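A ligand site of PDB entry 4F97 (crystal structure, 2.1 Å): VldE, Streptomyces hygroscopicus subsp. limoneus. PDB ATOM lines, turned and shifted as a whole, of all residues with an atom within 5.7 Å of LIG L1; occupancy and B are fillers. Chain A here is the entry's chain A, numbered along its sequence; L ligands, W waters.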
ATOM      1  N   LYS A  11      12.404  -8.399  21.074  1.00  0.00           N
ATOM      2  CA  LYS A  11      11.115  -7.714  21.025  1.00  0.00           C
ATOM      3  C   LYS A  11      10.709  -7.178  22.391  1.00  0.00           C
ATOM      4  O   LYS A  11      10.364  -6.001  22.518  1.00  0.00           O
ATOM      5  CB  LYS A  11      10.036  -8.654  20.487  1.00  0.00           C
ATOM      6  CG  LYS A  11       8.631  -8.113  20.650  1.00  0.00           C
ATOM      7  CD  LYS A  11       7.724  -8.558  19.515  1.00  0.00           C
ATOM      8  CE  LYS A  11       6.354  -7.904  19.605  1.00  0.00           C
ATOM      9  NZ  LYS A  11       5.475  -8.581  20.600  1.00  0.00           N
ATOM     10  N   TRP A 105       3.759 -16.893  12.594  1.00  0.00           N
ATOM     11  CA  TRP A 105       3.713 -18.052  13.514  1.00  0.00           C
ATOM     12  C   TRP A 105       3.272 -19.323  12.771  1.00  0.00           C
ATOM     13  O   TRP A 105       3.872 -20.362  12.934  1.00  0.00           O
ATOM     14  CB  TRP A 105       2.754 -17.803  14.677  1.00  0.00           C
ATOM     15  CG  TRP A 105       2.881 -18.828  15.782  1.00  0.00           C
ATOM     16  CD1 TRP A 105       2.025 -19.826  16.062  1.00  0.00           C
ATOM     17  CD2 TRP A 105       3.952 -18.946  16.710  1.00  0.00           C
ATOM     18  NE1 TRP A 105       2.455 -20.553  17.143  1.00  0.00           N
ATOM     19  CE2 TRP A 105       3.651 -20.015  17.566  1.00  0.00           C
ATOM     20  CE3 TRP A 105       5.130 -18.215  16.931  1.00  0.00           C
ATOM     21  CZ2 TRP A 105       4.493 -20.399  18.610  1.00  0.00           C
ATOM     22  CZ3 TRP A 105       5.949 -18.579  17.997  1.00  0.00           C
ATOM     23  CH2 TRP A 105       5.641 -19.674  18.787  1.00  0.00           C
ATOM     24  N   ASN A 109       5.781 -22.507  12.442  1.00  0.00           N
ATOM     25  CA  ASN A 109       5.307 -23.519  13.369  1.00  0.00           C
ATOM     26  C   ASN A 109       4.266 -24.441  12.746  1.00  0.00           C
ATOM     27  O   ASN A 109       3.462 -25.087  13.467  1.00  0.00           O
ATOM     28  CB  ASN A 109       4.742 -22.935  14.678  1.00  0.00           C
ATOM     29  CG  ASN A 109       5.786 -22.217  15.540  1.00  0.00           C
ATOM     30  OD1 ASN A 109       5.968 -21.056  15.476  1.00  0.00           O
ATOM     31  ND2 ASN A 109       6.382 -22.871  16.348  1.00  0.00           N
ATOM     32  N   ASP A 158      15.477 -13.663  18.449  1.00  0.00           N
ATOM     33  CA  ASP A 158      14.136 -14.114  18.052  1.00  0.00           C
ATOM     34  C   ASP A 158      13.653 -13.655  16.671  1.00  0.00           C
ATOM     35  O   ASP A 158      14.239 -12.772  16.058  1.00  0.00           O
ATOM     36  CB  ASP A 158      13.077 -13.871  19.135  1.00  0.00           C
ATOM     37  CG  ASP A 158      12.229 -15.111  19.399  1.00  0.00           C
ATOM     38  OD1 ASP A 158      12.145 -15.976  18.503  1.00  0.00           O
ATOM     39  OD2 ASP A 158      11.652 -15.222  20.504  1.00  0.00           O
ATOM     40  N   TYR A 159      12.556 -14.261  16.228  1.00  0.00           N
ATOM     41  CA  TYR A 159      12.074 -14.120  14.858  1.00  0.00           C
ATOM     42  C   TYR A 159      11.633 -12.711  14.459  1.00  0.00           C
ATOM     43  O   TYR A 159      11.839 -12.304  13.317  1.00  0.00           O
ATOM     44  CB  TYR A 159      11.009 -15.176  14.497  1.00  0.00           C
ATOM     45  CG  TYR A 159       9.727 -15.119  15.282  1.00  0.00           C
ATOM     46  CD1 TYR A 159       9.713 -15.278  16.665  1.00  0.00           C
ATOM     47  CD2 TYR A 159       8.505 -14.938  14.638  1.00  0.00           C
ATOM     48  CE1 TYR A 159       8.527 -15.237  17.378  1.00  0.00           C
ATOM     49  CE2 TYR A 159       7.317 -14.900  15.342  1.00  0.00           C
ATOM     50  CZ  TYR A 159       7.345 -15.046  16.713  1.00  0.00           C
ATOM     51  OH  TYR A 159       6.157 -15.008  17.416  1.00  0.00           O
ATOM     52  N   GLN A 160      11.018 -11.980  15.385  1.00  0.00           N
ATOM     53  CA  GLN A 160      10.546 -10.636  15.090  1.00  0.00           C
ATOM     54  C   GLN A 160      11.678  -9.747  14.570  1.00  0.00           C
ATOM     55  O   GLN A 160      11.420  -8.766  13.838  1.00  0.00           O
ATOM     56  CB  GLN A 160       9.915  -9.997  16.330  1.00  0.00           C
ATOM     57  CG  GLN A 160       8.687 -10.717  16.902  1.00  0.00           C
ATOM     58  CD  GLN A 160       9.029 -11.795  17.936  1.00  0.00           C
ATOM     59  OE1 GLN A 160      10.173 -12.234  18.033  1.00  0.00           O
ATOM     60  NE2 GLN A 160       8.026 -12.245  18.684  1.00  0.00           N
ATOM     61  N   HIS A 182      14.244 -18.532  18.123  1.00  0.00           N
ATOM     62  CA  HIS A 182      13.769 -19.345  19.240  1.00  0.00           C
ATOM     63  C   HIS A 182      12.723 -20.362  18.836  1.00  0.00           C
ATOM     64  O   HIS A 182      12.277 -21.152  19.660  1.00  0.00           O
ATOM     65  CB  HIS A 182      13.209 -18.453  20.362  1.00  0.00           C
ATOM     66  CG  HIS A 182      14.262 -17.703  21.141  1.00  0.00           C
ATOM     67  ND1 HIS A 182      14.350 -17.804  22.521  1.00  0.00           N
ATOM     68  CD2 HIS A 182      15.188 -16.833  20.745  1.00  0.00           C
ATOM     69  CE1 HIS A 182      15.330 -16.995  22.929  1.00  0.00           C
ATOM     70  NE2 HIS A 182      15.848 -16.387  21.885  1.00  0.00           N
ATOM     71  N   ILE A 183      12.338 -20.313  17.566  1.00  0.00           N
ATOM     72  CA  ILE A 183      11.246 -21.120  17.058  1.00  0.00           C
ATOM     73  C   ILE A 183      11.765 -21.991  15.921  1.00  0.00           C
ATOM     74  O   ILE A 183      12.898 -21.858  15.530  1.00  0.00           O
ATOM     75  CB  ILE A 183      10.092 -20.223  16.517  1.00  0.00           C
ATOM     76  CG1 ILE A 183      10.578 -19.315  15.368  1.00  0.00           C
ATOM     77  CG2 ILE A 183       9.492 -19.326  17.636  1.00  0.00           C
ATOM     78  CD1 ILE A 183       9.443 -18.541  14.659  1.00  0.00           C
ATOM     79  N   PHE A 215      17.645 -23.679  18.231  1.00  0.00           N
ATOM     80  CA  PHE A 215      17.741 -24.603  19.355  1.00  0.00           C
ATOM     81  C   PHE A 215      18.045 -26.057  18.937  1.00  0.00           C
ATOM     82  O   PHE A 215      18.419 -26.841  19.781  1.00  0.00           O
ATOM     83  CB  PHE A 215      16.446 -24.580  20.159  1.00  0.00           C
ATOM     84  CG  PHE A 215      16.271 -23.345  20.999  1.00  0.00           C
ATOM     85  CD1 PHE A 215      17.220 -23.004  21.967  1.00  0.00           C
ATOM     86  CD2 PHE A 215      15.149 -22.537  20.855  1.00  0.00           C
ATOM     87  CE1 PHE A 215      17.028 -21.889  22.772  1.00  0.00           C
ATOM     88  CE2 PHE A 215      14.950 -21.435  21.685  1.00  0.00           C
ATOM     89  CZ  PHE A 215      15.903 -21.110  22.634  1.00  0.00           C
ATOM     90  N   LEU A 257      18.908 -24.909  24.729  1.00  0.00           N
ATOM     91  CA  LEU A 257      18.636 -24.291  26.027  1.00  0.00           C
ATOM     92  C   LEU A 257      17.635 -25.218  26.723  1.00  0.00           C
ATOM     93  O   LEU A 257      16.778 -25.853  26.053  1.00  0.00           O
ATOM     94  CB  LEU A 257      18.069 -22.864  25.862  1.00  0.00           C
ATOM     95  CG  LEU A 257      17.498 -22.206  27.127  1.00  0.00           C
ATOM     96  CD1 LEU A 257      18.557 -22.045  28.231  1.00  0.00           C
ATOM     97  CD2 LEU A 257      16.907 -20.828  26.779  1.00  0.00           C
ATOM     98  N   ARG A 290       1.055 -22.811  26.849  1.00  0.00           N
ATOM     99  CA  ARG A 290       0.255 -21.671  26.430  1.00  0.00           C
ATOM    100  C   ARG A 290      -0.940 -22.114  25.559  1.00  0.00           C
ATOM    101  O   ARG A 290      -0.944 -23.228  25.018  1.00  0.00           O
ATOM    102  CB  ARG A 290       1.095 -20.719  25.577  1.00  0.00           C
ATOM    103  CG  ARG A 290       2.103 -19.854  26.292  1.00  0.00           C
ATOM    104  CD  ARG A 290       2.838 -18.923  25.290  1.00  0.00           C
ATOM    105  NE  ARG A 290       3.648 -19.677  24.324  1.00  0.00           N
ATOM    106  CZ  ARG A 290       3.353 -19.862  23.029  1.00  0.00           C
ATOM    107  NH1 ARG A 290       2.282 -19.319  22.476  1.00  0.00           N
ATOM    108  NH2 ARG A 290       4.155 -20.589  22.268  1.00  0.00           N
ATOM    109  N   ILE A 294       0.069 -25.228  18.725  1.00  0.00           N
ATOM    110  CA  ILE A 294       1.208 -26.169  18.704  1.00  0.00           C
ATOM    111  C   ILE A 294       1.318 -27.007  19.984  1.00  0.00           C
ATOM    112  O   ILE A 294       2.019 -28.001  19.990  1.00  0.00           O
ATOM    113  CB  ILE A 294       2.570 -25.462  18.512  1.00  0.00           C
ATOM    114  CG1 ILE A 294       2.940 -24.638  19.747  1.00  0.00           C
ATOM    115  CG2 ILE A 294       2.605 -24.647  17.255  1.00  0.00           C
ATOM    116  CD1 ILE A 294       4.310 -24.010  19.663  1.00  0.00           C
ATOM    117  N   LYS A 295       0.696 -26.586  21.088  1.00  0.00           N
ATOM    118  CA  LYS A 295       0.921 -27.276  22.355  1.00  0.00           C
ATOM    119  C   LYS A 295       0.160 -28.581  22.382  1.00  0.00           C
ATOM    120  O   LYS A 295       0.478 -29.434  23.210  1.00  0.00           O
ATOM    121  CB  LYS A 295       0.492 -26.417  23.537  1.00  0.00           C
ATOM    122  CG  LYS A 295       1.257 -25.122  23.699  1.00  0.00           C
ATOM    123  CD  LYS A 295       2.762 -25.386  23.856  1.00  0.00           C
ATOM    124  CE  LYS A 295       3.580 -24.173  23.458  1.00  0.00           C
ATOM    125  NZ  LYS A 295       5.036 -24.369  23.519  1.00  0.00           N
ATOM    126  N   ASN A 325      -2.781 -16.722  26.193  1.00  0.00           N
ATOM    127  CA  ASN A 325      -1.844 -15.979  25.381  1.00  0.00           C
ATOM    128  C   ASN A 325      -2.364 -15.807  23.951  1.00  0.00           C
ATOM    129  O   ASN A 325      -2.835 -16.787  23.334  1.00  0.00           O
ATOM    130  CB  ASN A 325      -0.511 -16.738  25.404  1.00  0.00           C
ATOM    131  CG  ASN A 325       0.483 -16.242  24.356  1.00  0.00           C
ATOM    132  OD1 ASN A 325       0.110 -15.797  23.339  1.00  0.00           O
ATOM    133  ND2 ASN A 325       1.724 -16.346  24.615  1.00  0.00           N
ATOM    134  N   ARG A 326      -2.368 -14.576  23.456  1.00  0.00           N
ATOM    135  CA  ARG A 326      -2.768 -14.312  22.084  1.00  0.00           C
ATOM    136  C   ARG A 326      -4.158 -14.842  21.767  1.00  0.00           C
ATOM    137  O   ARG A 326      -4.404 -15.331  20.666  1.00  0.00           O
ATOM    138  CB  ARG A 326      -1.759 -14.925  21.118  1.00  0.00           C
ATOM    139  CG  ARG A 326      -0.571 -14.040  20.836  1.00  0.00           C
ATOM    140  CD  ARG A 326       0.363 -14.719  19.858  1.00  0.00           C
ATOM    141  NE  ARG A 326       1.739 -14.726  20.349  1.00  0.00           N
ATOM    142  CZ  ARG A 326       2.691 -15.500  19.866  1.00  0.00           C
ATOM    143  NH1 ARG A 326       2.439 -16.327  18.866  1.00  0.00           N
ATOM    144  NH2 ARG A 326       3.915 -15.444  20.369  1.00  0.00           N
ATOM    145  N   ASP A 383       7.738 -27.653  18.358  1.00  0.00           N
ATOM    146  CA  ASP A 383       8.194 -26.614  19.269  1.00  0.00           C
ATOM    147  C   ASP A 383       9.620 -26.181  18.950  1.00  0.00           C
ATOM    148  O   ASP A 383      10.443 -27.006  18.539  1.00  0.00           O
ATOM    149  CB  ASP A 383       8.090 -27.086  20.725  1.00  0.00           C
ATOM    150  CG  ASP A 383       7.248 -26.148  21.578  1.00  0.00           C
ATOM    151  OD1 ASP A 383       7.382 -24.920  21.418  1.00  0.00           O
ATOM    152  OD2 ASP A 383       6.468 -26.650  22.400  1.00  0.00           O
ATOM    153  N   GLY A 384       9.937 -24.903  19.156  1.00  0.00           N
ATOM    154  CA  GLY A 384      11.278 -24.424  18.900  1.00  0.00           C
ATOM    155  C   GLY A 384      12.253 -25.145  19.802  1.00  0.00           C
ATOM    156  O   GLY A 384      13.307 -25.613  19.361  1.00  0.00           O
ATOM    157  N   GLN A 385      11.878 -25.287  21.066  1.00  0.00           N
ATOM    158  CA  GLN A 385      12.628 -26.132  21.981  1.00  0.00           C
ATOM    159  C   GLN A 385      11.671 -26.815  22.954  1.00  0.00           C
ATOM    160  O   GLN A 385      11.531 -28.017  22.953  1.00  0.00           O
ATOM    161  CB  GLN A 385      13.650 -25.300  22.742  1.00  0.00           C
ATOM    162  CG  GLN A 385      14.532 -26.115  23.726  1.00  0.00           C
ATOM    163  CD  GLN A 385      15.516 -27.041  23.005  1.00  0.00           C
ATOM    164  OE1 GLN A 385      15.394 -27.342  21.797  1.00  0.00           O
ATOM    165  NE2 GLN A 385      16.506 -27.481  23.743  1.00  0.00           N
ATOM    166  N   ASN A 386      11.041 -25.984  23.769  1.00  0.00           N
ATOM    167  CA  ASN A 386      10.179 -26.407  24.845  1.00  0.00           C
ATOM    168  C   ASN A 386      11.046 -26.555  26.076  1.00  0.00           C
ATOM    169  O   ASN A 386      11.690 -27.578  26.289  1.00  0.00           O
ATOM    170  CB  ASN A 386       9.454 -27.712  24.529  1.00  0.00           C
ATOM    171  CG  ASN A 386       8.318 -27.981  25.501  1.00  0.00           C
ATOM    172  OD1 ASN A 386       8.531 -28.116  26.702  1.00  0.00           O
ATOM    173  ND2 ASN A 386       7.100 -28.042  24.978  1.00  0.00           N
ATOM    174  N   LEU A 387      11.050 -25.513  26.892  1.00  0.00           N
ATOM    175  CA  LEU A 387      11.794 -25.522  28.165  1.00  0.00           C
ATOM    176  C   LEU A 387      11.036 -26.273  29.262  1.00  0.00           C
ATOM    177  O   LEU A 387      11.615 -26.723  30.232  1.00  0.00           O
ATOM    178  CB  LEU A 387      12.064 -24.112  28.648  1.00  0.00           C
ATOM    179  CG  LEU A 387      12.679 -23.112  27.660  1.00  0.00           C
ATOM    180  CD1 LEU A 387      13.140 -21.791  28.357  1.00  0.00           C
ATOM    181  CD2 LEU A 387      13.808 -23.771  26.874  1.00  0.00           C
HETATM  182  O1  LIG L   1       2.484 -14.268  23.128  1.00  0.00           O
HETATM  183  P1  LIG L   1       3.984 -14.157  23.253  1.00  0.00           P
HETATM  184  O2  LIG L   1       4.627 -13.341  22.149  1.00  0.00           O
HETATM  185  O3  LIG L   1       4.473 -13.841  24.635  1.00  0.00           O
HETATM  186  O4  LIG L   1       4.517 -15.656  22.990  1.00  0.00           O
HETATM  187  C1  LIG L   1       5.298 -16.325  23.968  1.00  0.00           C
HETATM  188  C2  LIG L   1       6.625 -16.743  23.350  1.00  0.00           C
HETATM  189  C3  LIG L   1       6.415 -17.994  22.508  1.00  0.00           C
HETATM  190  C4  LIG L   1       7.213 -15.608  22.530  1.00  0.00           C
HETATM  191  O5  LIG L   1       7.484 -14.497  23.385  1.00  0.00           O
HETATM  192  C5  LIG L   1       8.495 -16.035  21.850  1.00  0.00           C
HETATM  193  O6  LIG L   1       8.985 -14.954  21.052  1.00  0.00           O
HETATM  194  C6  LIG L   1       8.260 -17.252  20.955  1.00  0.00           C
HETATM  195  O7  LIG L   1       9.490 -17.654  20.356  1.00  0.00           O
HETATM  196  C7  LIG L   1       7.660 -18.424  21.744  1.00  0.00           C
HETATM  197  N1  LIG L   1       8.640 -19.035  22.633  1.00  0.00           N
HETATM  198  C8  LIG L   1       9.790 -19.717  22.077  1.00  0.00           C
HETATM  199  C9  LIG L   1      10.953 -19.711  23.053  1.00  0.00           C
HETATM  200  C10 LIG L   1       9.432 -21.123  21.561  1.00  0.00           C
HETATM  201  O8  LIG L   1       8.026 -21.186  21.290  1.00  0.00           O
HETATM  202  C11 LIG L   1       9.778 -22.261  22.513  1.00  0.00           C
HETATM  203  O9  LIG L   1       9.583 -23.504  21.843  1.00  0.00           O
HETATM  204  C12 LIG L   1      11.234 -22.182  22.968  1.00  0.00           C
HETATM  205  O10 LIG L   1      11.445 -23.163  23.992  1.00  0.00           O
HETATM  206  C13 LIG L   1      11.557 -20.820  23.501  1.00  0.00           C
HETATM  207  C14 LIG L   1      12.616 -20.695  24.581  1.00  0.00           C
HETATM  208  O11 LIG L   1      13.158 -19.368  24.579  1.00  0.00           O
HETATM  209  P1  LG2 L   2       6.820 -21.446  24.900  1.00  0.00           P
HETATM  210  O1  LG2 L   2       5.577 -20.937  25.554  1.00  0.00           O
HETATM  211  O2  LG2 L   2       6.440 -21.823  23.442  1.00  0.00           O
HETATM  212  O3  LG2 L   2       8.019 -20.566  24.784  1.00  0.00           O
HETATM  213  O4  LG2 L   2       7.132 -22.864  25.602  1.00  0.00           O
HETATM  214  P2  LG2 L   2       8.277 -23.277  26.633  1.00  0.00           P
HETATM  215  O5  LG2 L   2       7.813 -24.600  27.192  1.00  0.00           O
HETATM  216  O6  LG2 L   2       9.689 -23.310  26.118  1.00  0.00           O
HETATM  217  O7  LG2 L   2       8.185 -22.070  27.710  1.00  0.00           O
HETATM  218  C1  LG2 L   2       7.190 -22.004  28.688  1.00  0.00           C
HETATM  219  C2  LG2 L   2       7.753 -21.152  29.832  1.00  0.00           C
HETATM  220  O8  LG2 L   2       6.712 -20.465  30.519  1.00  0.00           O
HETATM  221  C3  LG2 L   2       8.397 -22.038  30.874  1.00  0.00           C
HETATM  222  O9  LG2 L   2       9.519 -21.332  31.407  1.00  0.00           O
HETATM  223  C4  LG2 L   2       7.296 -22.272  31.884  1.00  0.00           C
HETATM  224  O10 LG2 L   2       7.744 -22.661  33.186  1.00  0.00           O
HETATM  225  C5  LG2 L   2       6.624 -20.910  31.872  1.00  0.00           C
HETATM  226  N1  LG2 L   2       5.232 -21.004  32.387  1.00  0.00           N
HETATM  227  C6  LG2 L   2       4.541 -22.107  32.703  1.00  0.00           C
HETATM  228  N2  LG2 L   2       3.313 -21.769  33.157  1.00  0.00           N
HETATM  229  C7  LG2 L   2       3.201 -20.430  33.126  1.00  0.00           C
HETATM  230  C8  LG2 L   2       2.175 -19.423  33.453  1.00  0.00           C
HETATM  231  O11 LG2 L   2       1.045 -19.764  33.885  1.00  0.00           O
HETATM  232  N3  LG2 L   2       2.447 -18.146  33.220  1.00  0.00           N
HETATM  233  C9  LG2 L   2       3.635 -17.726  32.760  1.00  0.00           C
HETATM  234  N4  LG2 L   2       3.876 -16.401  32.587  1.00  0.00           N
HETATM  235  N5  LG2 L   2       4.637 -18.601  32.453  1.00  0.00           N
HETATM  236  C10 LG2 L   2       4.463 -19.930  32.601  1.00  0.00           C
HETATM  237  O   HOH W   1       7.861 -22.684  18.835  1.00  0.00           O
HETATM  238  O   HOH W   2      10.063 -17.225  24.915  1.00  0.00           O
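Merely in contact with LIG L1: Ile 183, Arg 290, Tyr 159, Gln 160, Leu 387, Trp 105 and Phe 215. Hydrophobic or aromatic side chains that line LIG L1: Trp 105, Tyr 159, His 182, Ile 183, Phe 215 and Leu 387. Of the 20 residues printed, 15 come within 4 Å of LIG L1.
O1 of LIG L1 is in hydrogen-bond range of ND2 of Asn 325 (2.7 Å). OD2 of Asp 158 lies within hydrogen-bond range of O6 of LIG L1 (2.7 Å). The guanidinium group of Arg 326 lies within salt-bridge range of an oxygen (O2) of LIG L1, at 2.8 Å. O2 of LG2 L2 is in salt-bridge range of NZ of Lys 295 (2.9 Å). ND1 of His 182 lies within hydrogen-bond range of O11 of LIG L1, 2.8 Å away. An oxygen (O9) of LIG L1 sits at hydrogen-bond distance from the backbone NH (N) of Gly 384, at 3.0 Å. The side-chain carboxylate (OD1) of Asp 383 lies within hydrogen-bond range of an oxygen (O9) of LIG L1 (2.7 Å). An oxygen (O6) of LG2 L2 is in hydrogen-bond range of the backbone NH of Leu 387 (2.7 Å). NE of Arg 290 is in salt-bridge range of O1 of LG2 L2 (2.6 Å). The backbone NH (N) of Gln 385 is in hydrogen-bond range of an oxygen (O9) of LIG L1 (3.0 Å). An oxygen (O10) of LIG L1 lies within hydrogen-bond range of the backbone NH (N) of Asn 386, 2.9 Å away.
An oxygen (O3) of LG2 L2 is in hydrogen-bond range of a nitrogen (N1) of LIG L1 (2.7 Å).
OD2 of Asp 383 is in hydrogen-bond range of ND2 of Asn 386, 3.0 Å away. The backbone carbonyl oxygen (O) of Leu 257 lies within hydrogen-bond range of the side-chain amide nitrogen (NE2) of Gln 385 (2.8 Å). The side-chain amino group of Lys 295 is in salt-bridge range of the side-chain carboxylate of Asp 383, 2.9 Å away. The side-chain carboxylate (OD1) of Asp 158 sits close to the backbone NH (N) of His 182 (3.3 Å). The backbone carbonyl oxygen (O) of Trp 105 lies close to the side-chain amide oxygen (OD1) of Asn 109.
Water W1 lies within hydrogen-bond range of an oxygen (O8) of LIG L1 (2.9 Å), the side-chain amide nitrogen of Asn 109 (2.9 Å), the backbone NH of Gly 384 (3.1 Å) and the side-chain carboxylate of Asp 383 (3.4 Å).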
